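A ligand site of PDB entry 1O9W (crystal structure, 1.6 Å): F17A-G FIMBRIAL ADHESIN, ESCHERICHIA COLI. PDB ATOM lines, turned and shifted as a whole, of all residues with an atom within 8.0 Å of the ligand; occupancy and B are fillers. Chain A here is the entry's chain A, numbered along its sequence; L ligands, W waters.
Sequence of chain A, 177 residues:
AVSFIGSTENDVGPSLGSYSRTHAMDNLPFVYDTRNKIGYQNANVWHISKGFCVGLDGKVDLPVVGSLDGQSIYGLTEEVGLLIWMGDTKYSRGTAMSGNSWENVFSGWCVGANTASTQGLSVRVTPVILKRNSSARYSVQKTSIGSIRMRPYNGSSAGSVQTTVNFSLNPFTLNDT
OD2 of Asp 88 lies within hydrogen-bond range of O5 of the ligand (2.7 Å). An oxygen (O2) of the ligand lies within hydrogen-bond range of the backbone carbonyl oxygen (O) of Ala 43. The side-chain hydroxyl of Thr 89 is in hydrogen-bond range of an oxygen (O2) of the ligand (2.7 Å). The backbone NH (N) of Gly 120 is in hydrogen-bond range of an oxygen (O3) of the ligand (2.8 Å). OG1 of Thr 118 lies within hydrogen-bond range of N1 of the ligand (3.0 Å). The side-chain amide nitrogen (NE2) of Gln 119 is in hydrogen-bond range of an oxygen (O3) of the ligand, at 3.1 Å. The side-chain amide oxygen (OD1) of Asn 44 lies close to an oxygen (O6) of the ligand.
OD1 of Asp 88 sits at hydrogen-bond distance from NE2 of Gln 119, at 3.1 Å. N of Gly 120 lies within hydrogen-bond range of O of Ala 43, 3.2 Å away. The backbone NH (N) of Leu 121 sits at hydrogen-bond distance from the side-chain hydroxyl (OG1) of Thr 89. The backbone carbonyl oxygen (O) of Thr 89 sits at hydrogen-bond distance from the side-chain amide nitrogen (NE2) of Gln 41 (2.9 Å). OE1 of Gln 119 sits at hydrogen-bond distance from NE1 of Trp 109. N of Val 45 is in hydrogen-bond range of O of Gln 119. O of Trp 46 is in hydrogen-bond range of N of Gln 119 (2.8 Å). OD1 of Asn 42 is in hydrogen-bond range of N of Asn 44, 2.9 Å away.
NE1 of Trp 109 touches C6 of the ligand, at 3.2 Å. Ser 117 touches the ligand (OG to O1, 3.7 Å). Hydrophobic or aromatic side chains within 4 Å of the ligand: Ala 43 and Trp 109. Within 4 Å of the ligand: Ala 43, Asn 44, Asp 88, Thr 89, Trp 109, Ser 117, Thr 118, Gln 119 and Gly 120. Along chain A the residues within 4 Å of the ligand span positions 43 to 120.
Water W4 bridges O1 of the ligand (2.9 Å) and OG of Ser 117 (3.1 Å).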
ATOM      1  N   GLN A  41       3.101  19.569  33.376  1.00  0.00           N
ATOM      2  CA  GLN A  41       3.818  20.193  32.298  1.00  0.00           C
ATOM      3  C   GLN A  41       3.230  19.696  31.000  1.00  0.00           C
ATOM      4  O   GLN A  41       2.956  18.493  30.871  1.00  0.00           O
ATOM      5  CB  GLN A  41       5.278  19.790  32.432  1.00  0.00           C
ATOM      6  CG  GLN A  41       6.141  20.046  31.256  1.00  0.00           C
ATOM      7  CD  GLN A  41       7.564  19.609  31.539  1.00  0.00           C
ATOM      8  OE1 GLN A  41       7.877  18.411  31.610  1.00  0.00           O
ATOM      9  NE2 GLN A  41       8.420  20.583  31.759  1.00  0.00           N
ATOM     10  N   ASN A  42       3.032  20.610  30.068  1.00  0.00           N
ATOM     11  CA  ASN A  42       2.502  20.249  28.758  1.00  0.00           C
ATOM     12  C   ASN A  42       3.030  21.271  27.764  1.00  0.00           C
ATOM     13  O   ASN A  42       2.683  22.446  27.822  1.00  0.00           O
ATOM     14  CB  ASN A  42       0.975  20.295  28.790  1.00  0.00           C
ATOM     15  CG  ASN A  42       0.347  19.849  27.471  1.00  0.00           C
ATOM     16  OD1 ASN A  42       1.028  19.631  26.452  1.00  0.00           O
ATOM     17  ND2 ASN A  42      -0.966  19.732  27.472  1.00  0.00           N
ATOM     18  N   ALA A  43       3.906  20.833  26.863  1.00  0.00           N
ATOM     19  CA  ALA A  43       4.476  21.734  25.884  1.00  0.00           C
ATOM     20  C   ALA A  43       3.485  22.233  24.866  1.00  0.00           C
ATOM     21  O   ALA A  43       3.755  23.229  24.187  1.00  0.00           O
ATOM     22  CB  ALA A  43       5.645  21.079  25.185  1.00  0.00           C
ATOM     23  N   ASN A  44       2.314  21.591  24.789  1.00  0.00           N
ATOM     24  CA  ASN A  44       1.384  21.941  23.744  1.00  0.00           C
ATOM     25  C   ASN A  44      -0.025  22.208  24.222  1.00  0.00           C
ATOM     26  O   ASN A  44      -0.870  21.307  24.234  1.00  0.00           O
ATOM     27  CB  ASN A  44       1.421  20.801  22.710  1.00  0.00           C
ATOM     28  CG  ASN A  44       2.845  20.247  22.522  1.00  0.00           C
ATOM     29  OD1 ASN A  44       3.736  20.925  22.005  1.00  0.00           O
ATOM     30  ND2 ASN A  44       3.070  19.003  22.955  1.00  0.00           N
ATOM     31  N   VAL A  45      -0.280  23.442  24.648  1.00  0.00           N
ATOM     32  CA  VAL A  45      -1.598  23.808  25.104  1.00  0.00           C
ATOM     33  C   VAL A  45      -2.320  24.640  24.033  1.00  0.00           C
ATOM     34  O   VAL A  45      -3.546  24.561  23.890  1.00  0.00           O
ATOM     35  CB  VAL A  45      -1.520  24.522  26.483  1.00  0.00           C
ATOM     36  CG1 VAL A  45      -2.904  24.926  26.975  1.00  0.00           C
ATOM     37  CG2 VAL A  45      -0.842  23.552  27.478  1.00  0.00           C
ATOM     38  N   TRP A  46      -1.555  25.434  23.280  1.00  0.00           N
ATOM     39  CA  TRP A  46      -2.095  26.220  22.174  1.00  0.00           C
ATOM     40  C   TRP A  46      -1.186  25.990  20.982  1.00  0.00           C
ATOM     41  O   TRP A  46       0.034  25.813  21.134  1.00  0.00           O
ATOM     42  CB  TRP A  46      -2.096  27.739  22.494  1.00  0.00           C
ATOM     43  CG  TRP A  46      -3.057  28.131  23.546  1.00  0.00           C
ATOM     44  CD1 TRP A  46      -4.395  28.370  23.395  1.00  0.00           C
ATOM     45  CD2 TRP A  46      -2.779  28.235  24.949  1.00  0.00           C
ATOM     46  NE1 TRP A  46      -4.969  28.628  24.623  1.00  0.00           N
ATOM     47  CE2 TRP A  46      -4.002  28.544  25.595  1.00  0.00           C
ATOM     48  CE3 TRP A  46      -1.617  28.088  25.727  1.00  0.00           C
ATOM     49  CZ2 TRP A  46      -4.105  28.709  26.972  1.00  0.00           C
ATOM     50  CZ3 TRP A  46      -1.715  28.266  27.103  1.00  0.00           C
ATOM     51  CH2 TRP A  46      -2.950  28.566  27.710  1.00  0.00           C
ATOM     52  N   ILE A  48       0.202  27.748  17.716  1.00  0.00           N
ATOM     53  CA  ILE A  48       0.324  29.124  17.217  1.00  0.00           C
ATOM     54  C   ILE A  48       1.124  29.200  15.935  1.00  0.00           C
ATOM     55  O   ILE A  48       1.978  28.360  15.683  1.00  0.00           O
ATOM     56  CB  ILE A  48       0.972  30.067  18.248  1.00  0.00           C
ATOM     57  CG1 ILE A  48       2.371  29.591  18.573  1.00  0.00           C
ATOM     58  CG2 ILE A  48       0.106  30.129  19.511  1.00  0.00           C
ATOM     59  CD1 ILE A  48       3.134  30.516  19.577  1.00  0.00           C
ATOM     60  N   VAL A  54       2.738  35.492  22.067  1.00  0.00           N
ATOM     61  CA  VAL A  54       1.999  35.107  23.270  1.00  0.00           C
ATOM     62  C   VAL A  54       2.868  34.854  24.520  1.00  0.00           C
ATOM     63  O   VAL A  54       4.011  34.371  24.450  1.00  0.00           O
ATOM     64  CB  VAL A  54       1.148  33.798  22.958  1.00  0.00           C
ATOM     65  CG1 VAL A  54       2.080  32.651  22.689  1.00  0.00           C
ATOM     66  CG2 VAL A  54       0.170  33.480  24.079  1.00  0.00           C
ATOM     67  N   LEU A  56       2.151  34.260  29.166  1.00  0.00           N
ATOM     68  CA  LEU A  56       1.227  33.596  30.084  1.00  0.00           C
ATOM     69  C   LEU A  56       1.013  34.379  31.371  1.00  0.00           C
ATOM     70  O   LEU A  56       1.943  34.985  31.908  1.00  0.00           O
ATOM     71  CB  LEU A  56       1.766  32.212  30.500  1.00  0.00           C
ATOM     72  CG  LEU A  56       2.031  31.154  29.426  1.00  0.00           C
ATOM     73  CD1 LEU A  56       2.826  29.992  30.062  1.00  0.00           C
ATOM     74  CD2 LEU A  56       0.664  30.656  28.828  1.00  0.00           C
ATOM     75  N   GLY A  87       4.468  28.865  34.885  1.00  0.00           N
ATOM     76  CA  GLY A  87       5.246  29.509  33.843  1.00  0.00           C
ATOM     77  C   GLY A  87       5.206  28.760  32.538  1.00  0.00           C
ATOM     78  O   GLY A  87       4.310  27.953  32.310  1.00  0.00           O
ATOM     79  N   ASP A  88       6.204  29.047  31.697  1.00  0.00           N
ATOM     80  CA  ASP A  88       6.335  28.387  30.413  1.00  0.00           C
ATOM     81  C   ASP A  88       6.616  26.888  30.641  1.00  0.00           C
ATOM     82  O   ASP A  88       6.867  26.413  31.759  1.00  0.00           O
ATOM     83  CB  ASP A  88       7.470  29.050  29.633  1.00  0.00           C
ATOM     84  CG  ASP A  88       7.506  28.656  28.172  1.00  0.00           C
ATOM     85  OD1 ASP A  88       6.467  28.243  27.619  1.00  0.00           O
ATOM     86  OD2 ASP A  88       8.599  28.793  27.569  1.00  0.00           O
ATOM     87  N   THR A  89       6.582  26.135  29.557  1.00  0.00           N
ATOM     88  CA  THR A  89       6.783  24.697  29.611  1.00  0.00           C
ATOM     89  C   THR A  89       7.873  24.127  30.509  1.00  0.00           C
ATOM     90  O   THR A  89       7.584  23.325  31.386  1.00  0.00           O
ATOM     91  CB  THR A  89       6.986  24.189  28.182  1.00  0.00           C
ATOM     92  OG1 THR A  89       5.882  24.635  27.413  1.00  0.00           O
ATOM     93  CG2 THR A  89       7.120  22.656  28.141  1.00  0.00           C
ATOM     94  N   LYS A  90       9.122  24.534  30.318  1.00  0.00           N
ATOM     95  CA  LYS A  90      10.201  23.924  31.104  1.00  0.00           C
ATOM     96  C   LYS A  90      10.137  24.396  32.557  1.00  0.00           C
ATOM     97  O   LYS A  90       9.985  25.591  32.819  1.00  0.00           O
ATOM     98  CB  LYS A  90      11.564  24.231  30.442  1.00  0.00           C
ATOM     99  CG  LYS A  90      11.714  23.471  29.093  1.00  0.00           C
ATOM    100  CD  LYS A  90      13.132  23.428  28.597  1.00  0.00           C
ATOM    101  CE  LYS A  90      13.245  22.675  27.252  1.00  0.00           C
ATOM    102  NZ  LYS A  90      13.043  23.585  26.104  1.00  0.00           N
ATOM    103  N   ARG A  93      11.739  27.524  34.057  1.00  0.00           N
ATOM    104  CA  ARG A  93      11.214  28.845  33.673  1.00  0.00           C
ATOM    105  C   ARG A  93      10.079  29.286  34.583  1.00  0.00           C
ATOM    106  O   ARG A  93       9.511  30.341  34.373  1.00  0.00           O
ATOM    107  CB  ARG A  93      10.659  28.830  32.246  1.00  0.00           C
ATOM    108  CG  ARG A  93      11.593  28.208  31.227  1.00  0.00           C
ATOM    109  CD  ARG A  93      12.882  28.988  31.078  1.00  0.00           C
ATOM    110  NE  ARG A  93      13.931  28.162  30.468  1.00  0.00           N
ATOM    111  CZ  ARG A  93      13.923  27.743  29.203  1.00  0.00           C
ATOM    112  NH1 ARG A  93      14.919  26.996  28.742  1.00  0.00           N
ATOM    113  NH2 ARG A  93      12.940  28.106  28.388  1.00  0.00           N
ATOM    114  N   PHE A 106       5.147  34.372  32.319  1.00  0.00           N
ATOM    115  CA  PHE A 106       5.970  34.137  31.135  1.00  0.00           C
ATOM    116  C   PHE A 106       5.860  35.382  30.240  1.00  0.00           C
ATOM    117  O   PHE A 106       4.791  35.702  29.710  1.00  0.00           O
ATOM    118  CB  PHE A 106       5.513  32.868  30.382  1.00  0.00           C
ATOM    119  CG  PHE A 106       6.247  32.647  29.098  1.00  0.00           C
ATOM    120  CD1 PHE A 106       7.640  32.757  29.044  1.00  0.00           C
ATOM    121  CD2 PHE A 106       5.567  32.288  27.938  1.00  0.00           C
ATOM    122  CE1 PHE A 106       8.344  32.518  27.877  1.00  0.00           C
ATOM    123  CE2 PHE A 106       6.261  32.042  26.750  1.00  0.00           C
ATOM    124  CZ  PHE A 106       7.650  32.157  26.719  1.00  0.00           C
ATOM    125  N   GLY A 108       6.824  35.908  27.331  1.00  0.00           N
ATOM    126  CA  GLY A 108       6.366  35.642  25.967  1.00  0.00           C
ATOM    127  C   GLY A 108       7.333  35.556  24.821  1.00  0.00           C
ATOM    128  O   GLY A 108       8.524  35.815  24.954  1.00  0.00           O
ATOM    129  N   TRP A 109       6.814  35.144  23.670  1.00  0.00           N
ATOM    130  CA  TRP A 109       7.615  35.036  22.456  1.00  0.00           C
ATOM    131  C   TRP A 109       6.680  35.118  21.275  1.00  0.00           C
ATOM    132  O   TRP A 109       5.458  35.022  21.420  1.00  0.00           O
ATOM    133  CB  TRP A 109       8.369  33.705  22.409  1.00  0.00           C
ATOM    134  CG  TRP A 109       7.506  32.494  22.108  1.00  0.00           C
ATOM    135  CD1 TRP A 109       6.494  31.973  22.876  1.00  0.00           C
ATOM    136  CD2 TRP A 109       7.687  31.587  21.006  1.00  0.00           C
ATOM    137  NE1 TRP A 109       6.047  30.794  22.314  1.00  0.00           N
ATOM    138  CE2 TRP A 109       6.764  30.538  21.170  1.00  0.00           C
ATOM    139  CE3 TRP A 109       8.549  31.570  19.898  1.00  0.00           C
ATOM    140  CZ2 TRP A 109       6.668  29.468  20.267  1.00  0.00           C
ATOM    141  CZ3 TRP A 109       8.452  30.500  18.995  1.00  0.00           C
ATOM    142  CH2 TRP A 109       7.526  29.464  19.194  1.00  0.00           C
ATOM    143  N   CYS A 110       7.248  35.295  20.084  1.00  0.00           N
ATOM    144  CA  CYS A 110       6.422  35.346  18.878  1.00  0.00           C
ATOM    145  C   CYS A 110       6.943  34.268  17.938  1.00  0.00           C
ATOM    146  O   CYS A 110       8.156  34.161  17.740  1.00  0.00           O
ATOM    147  CB  CYS A 110       6.551  36.673  18.153  1.00  0.00           C
ATOM    148  SG  CYS A 110       6.173  38.159  19.128  1.00  0.00           S
ATOM    149  N   VAL A 111       6.037  33.466  17.378  1.00  0.00           N
ATOM    150  CA  VAL A 111       6.439  32.421  16.453  1.00  0.00           C
ATOM    151  C   VAL A 111       6.667  33.155  15.122  1.00  0.00           C
ATOM    152  O   VAL A 111       6.217  34.284  14.947  1.00  0.00           O
ATOM    153  CB  VAL A 111       5.321  31.345  16.308  1.00  0.00           C
ATOM    154  CG1 VAL A 111       4.045  31.937  15.728  1.00  0.00           C
ATOM    155  CG2 VAL A 111       5.820  30.194  15.447  1.00  0.00           C
ATOM    156  N   ALA A 116       4.999  27.610  12.228  1.00  0.00           N
ATOM    157  CA  ALA A 116       4.069  27.251  13.299  1.00  0.00           C
ATOM    158  C   ALA A 116       4.780  26.502  14.378  1.00  0.00           C
ATOM    159  O   ALA A 116       5.801  25.866  14.126  1.00  0.00           O
ATOM    160  CB  ALA A 116       2.963  26.373  12.727  1.00  0.00           C
ATOM    161  N   SER A 117       4.211  26.540  15.575  1.00  0.00           N
ATOM    162  CA  SER A 117       4.754  25.817  16.711  1.00  0.00           C
ATOM    163  C   SER A 117       3.665  25.748  17.771  1.00  0.00           C
ATOM    164  O   SER A 117       2.474  25.901  17.465  1.00  0.00           O
ATOM    165  CB  SER A 117       6.013  26.512  17.263  1.00  0.00           C
ATOM    166  OG  SER A 117       6.659  25.653  18.196  1.00  0.00           O
ATOM    167  N   THR A 118       4.055  25.513  19.026  1.00  0.00           N
ATOM    168  CA  THR A 118       3.077  25.449  20.104  1.00  0.00           C
ATOM    169  C   THR A 118       3.524  26.263  21.303  1.00  0.00           C
ATOM    170  O   THR A 118       4.698  26.609  21.404  1.00  0.00           O
ATOM    171  CB  THR A 118       2.873  24.008  20.615  1.00  0.00           C
ATOM    172  OG1 THR A 118       4.118  23.441  21.074  1.00  0.00           O
ATOM    173  CG2 THR A 118       2.338  23.114  19.475  1.00  0.00           C
ATOM    174  N   GLN A 119       2.561  26.589  22.144  1.00  0.00           N
ATOM    175  CA  GLN A 119       2.795  27.303  23.406  1.00  0.00           C
ATOM    176  C   GLN A 119       2.346  26.358  24.517  1.00  0.00           C
ATOM    177  O   GLN A 119       1.204  25.864  24.482  1.00  0.00           O
ATOM    178  CB  GLN A 119       1.949  28.588  23.476  1.00  0.00           C
ATOM    179  CG  GLN A 119       2.069  29.327  24.823  1.00  0.00           C
ATOM    180  CD  GLN A 119       3.494  29.655  25.175  1.00  0.00           C
ATOM    181  OE1 GLN A 119       4.255  30.179  24.332  1.00  0.00           O
ATOM    182  NE2 GLN A 119       3.882  29.374  26.421  1.00  0.00           N
ATOM    183  N   GLY A 120       3.232  26.138  25.493  1.00  0.00           N
ATOM    184  CA  GLY A 120       2.910  25.257  26.592  1.00  0.00           C
ATOM    185  C   GLY A 120       2.934  25.956  27.939  1.00  0.00           C
ATOM    186  O   GLY A 120       2.857  27.182  28.018  1.00  0.00           O
ATOM    187  N   LEU A 121       3.055  25.166  29.001  1.00  0.00           N
ATOM    188  CA  LEU A 121       3.066  25.746  30.335  1.00  0.00           C
ATOM    189  C   LEU A 121       3.444  24.708  31.379  1.00  0.00           C
ATOM    190  O   LEU A 121       3.509  23.518  31.071  1.00  0.00           O
ATOM    191  CB  LEU A 121       1.681  26.307  30.681  1.00  0.00           C
ATOM    192  CG  LEU A 121       0.452  25.391  30.446  1.00  0.00           C
ATOM    193  CD1 LEU A 121       0.339  24.289  31.526  1.00  0.00           C
ATOM    194  CD2 LEU A 121      -0.813  26.232  30.430  1.00  0.00           C
ATOM    195  N   SER A 122       3.727  25.175  32.595  1.00  0.00           N
ATOM    196  CA  SER A 122       4.044  24.258  33.679  1.00  0.00           C
ATOM    197  C   SER A 122       3.582  24.845  35.000  1.00  0.00           C
ATOM    198  O   SER A 122       3.529  26.077  35.146  1.00  0.00           O
ATOM    199  CB  SER A 122       5.556  23.970  33.791  1.00  0.00           C
ATOM    200  OG  SER A 122       6.299  25.128  34.148  1.00  0.00           O
HETATM  201  C1  LIG L   1       7.956  26.090  21.882  1.00  0.00           C
HETATM  202  C2  LIG L   1       7.498  24.937  22.788  1.00  0.00           C
HETATM  203  C3  LIG L   1       6.423  25.432  23.760  1.00  0.00           C
HETATM  204  C4  LIG L   1       6.895  26.687  24.506  1.00  0.00           C
HETATM  205  C5  LIG L   1       7.369  27.729  23.507  1.00  0.00           C
HETATM  206  C6  LIG L   1       7.905  28.993  24.161  1.00  0.00           C
HETATM  207  C7  LIG L   1       7.447  22.670  21.866  1.00  0.00           C
HETATM  208  C8  LIG L   1       8.648  22.307  22.690  1.00  0.00           C
HETATM  209  N1  LIG L   1       6.918  23.889  21.959  1.00  0.00           N
HETATM  210  O1  LIG L   1       9.015  25.675  21.110  1.00  0.00           O
HETATM  211  O2  LIG L   1       6.080  24.414  24.697  1.00  0.00           O
HETATM  212  O3  LIG L   1       5.810  27.208  25.256  1.00  0.00           O
HETATM  213  O4  LIG L   1       8.420  27.183  22.706  1.00  0.00           O
HETATM  214  O5  LIG L   1       9.041  28.689  24.950  1.00  0.00           O
HETATM  215  O6  LIG L   1       6.971  21.790  21.115  1.00  0.00           O
HETATM  216  O   HOH W   1      10.386  29.019  21.345  1.00  0.00           O
HETATM  217  O   HOH W   2      11.203  27.587  24.357  1.00  0.00           O
HETATM  218  O   HOH W   3      11.131  25.115  22.653  1.00  0.00           O
HETATM  219  O   HOH W   4       9.665  26.182  18.348  1.00  0.00           O
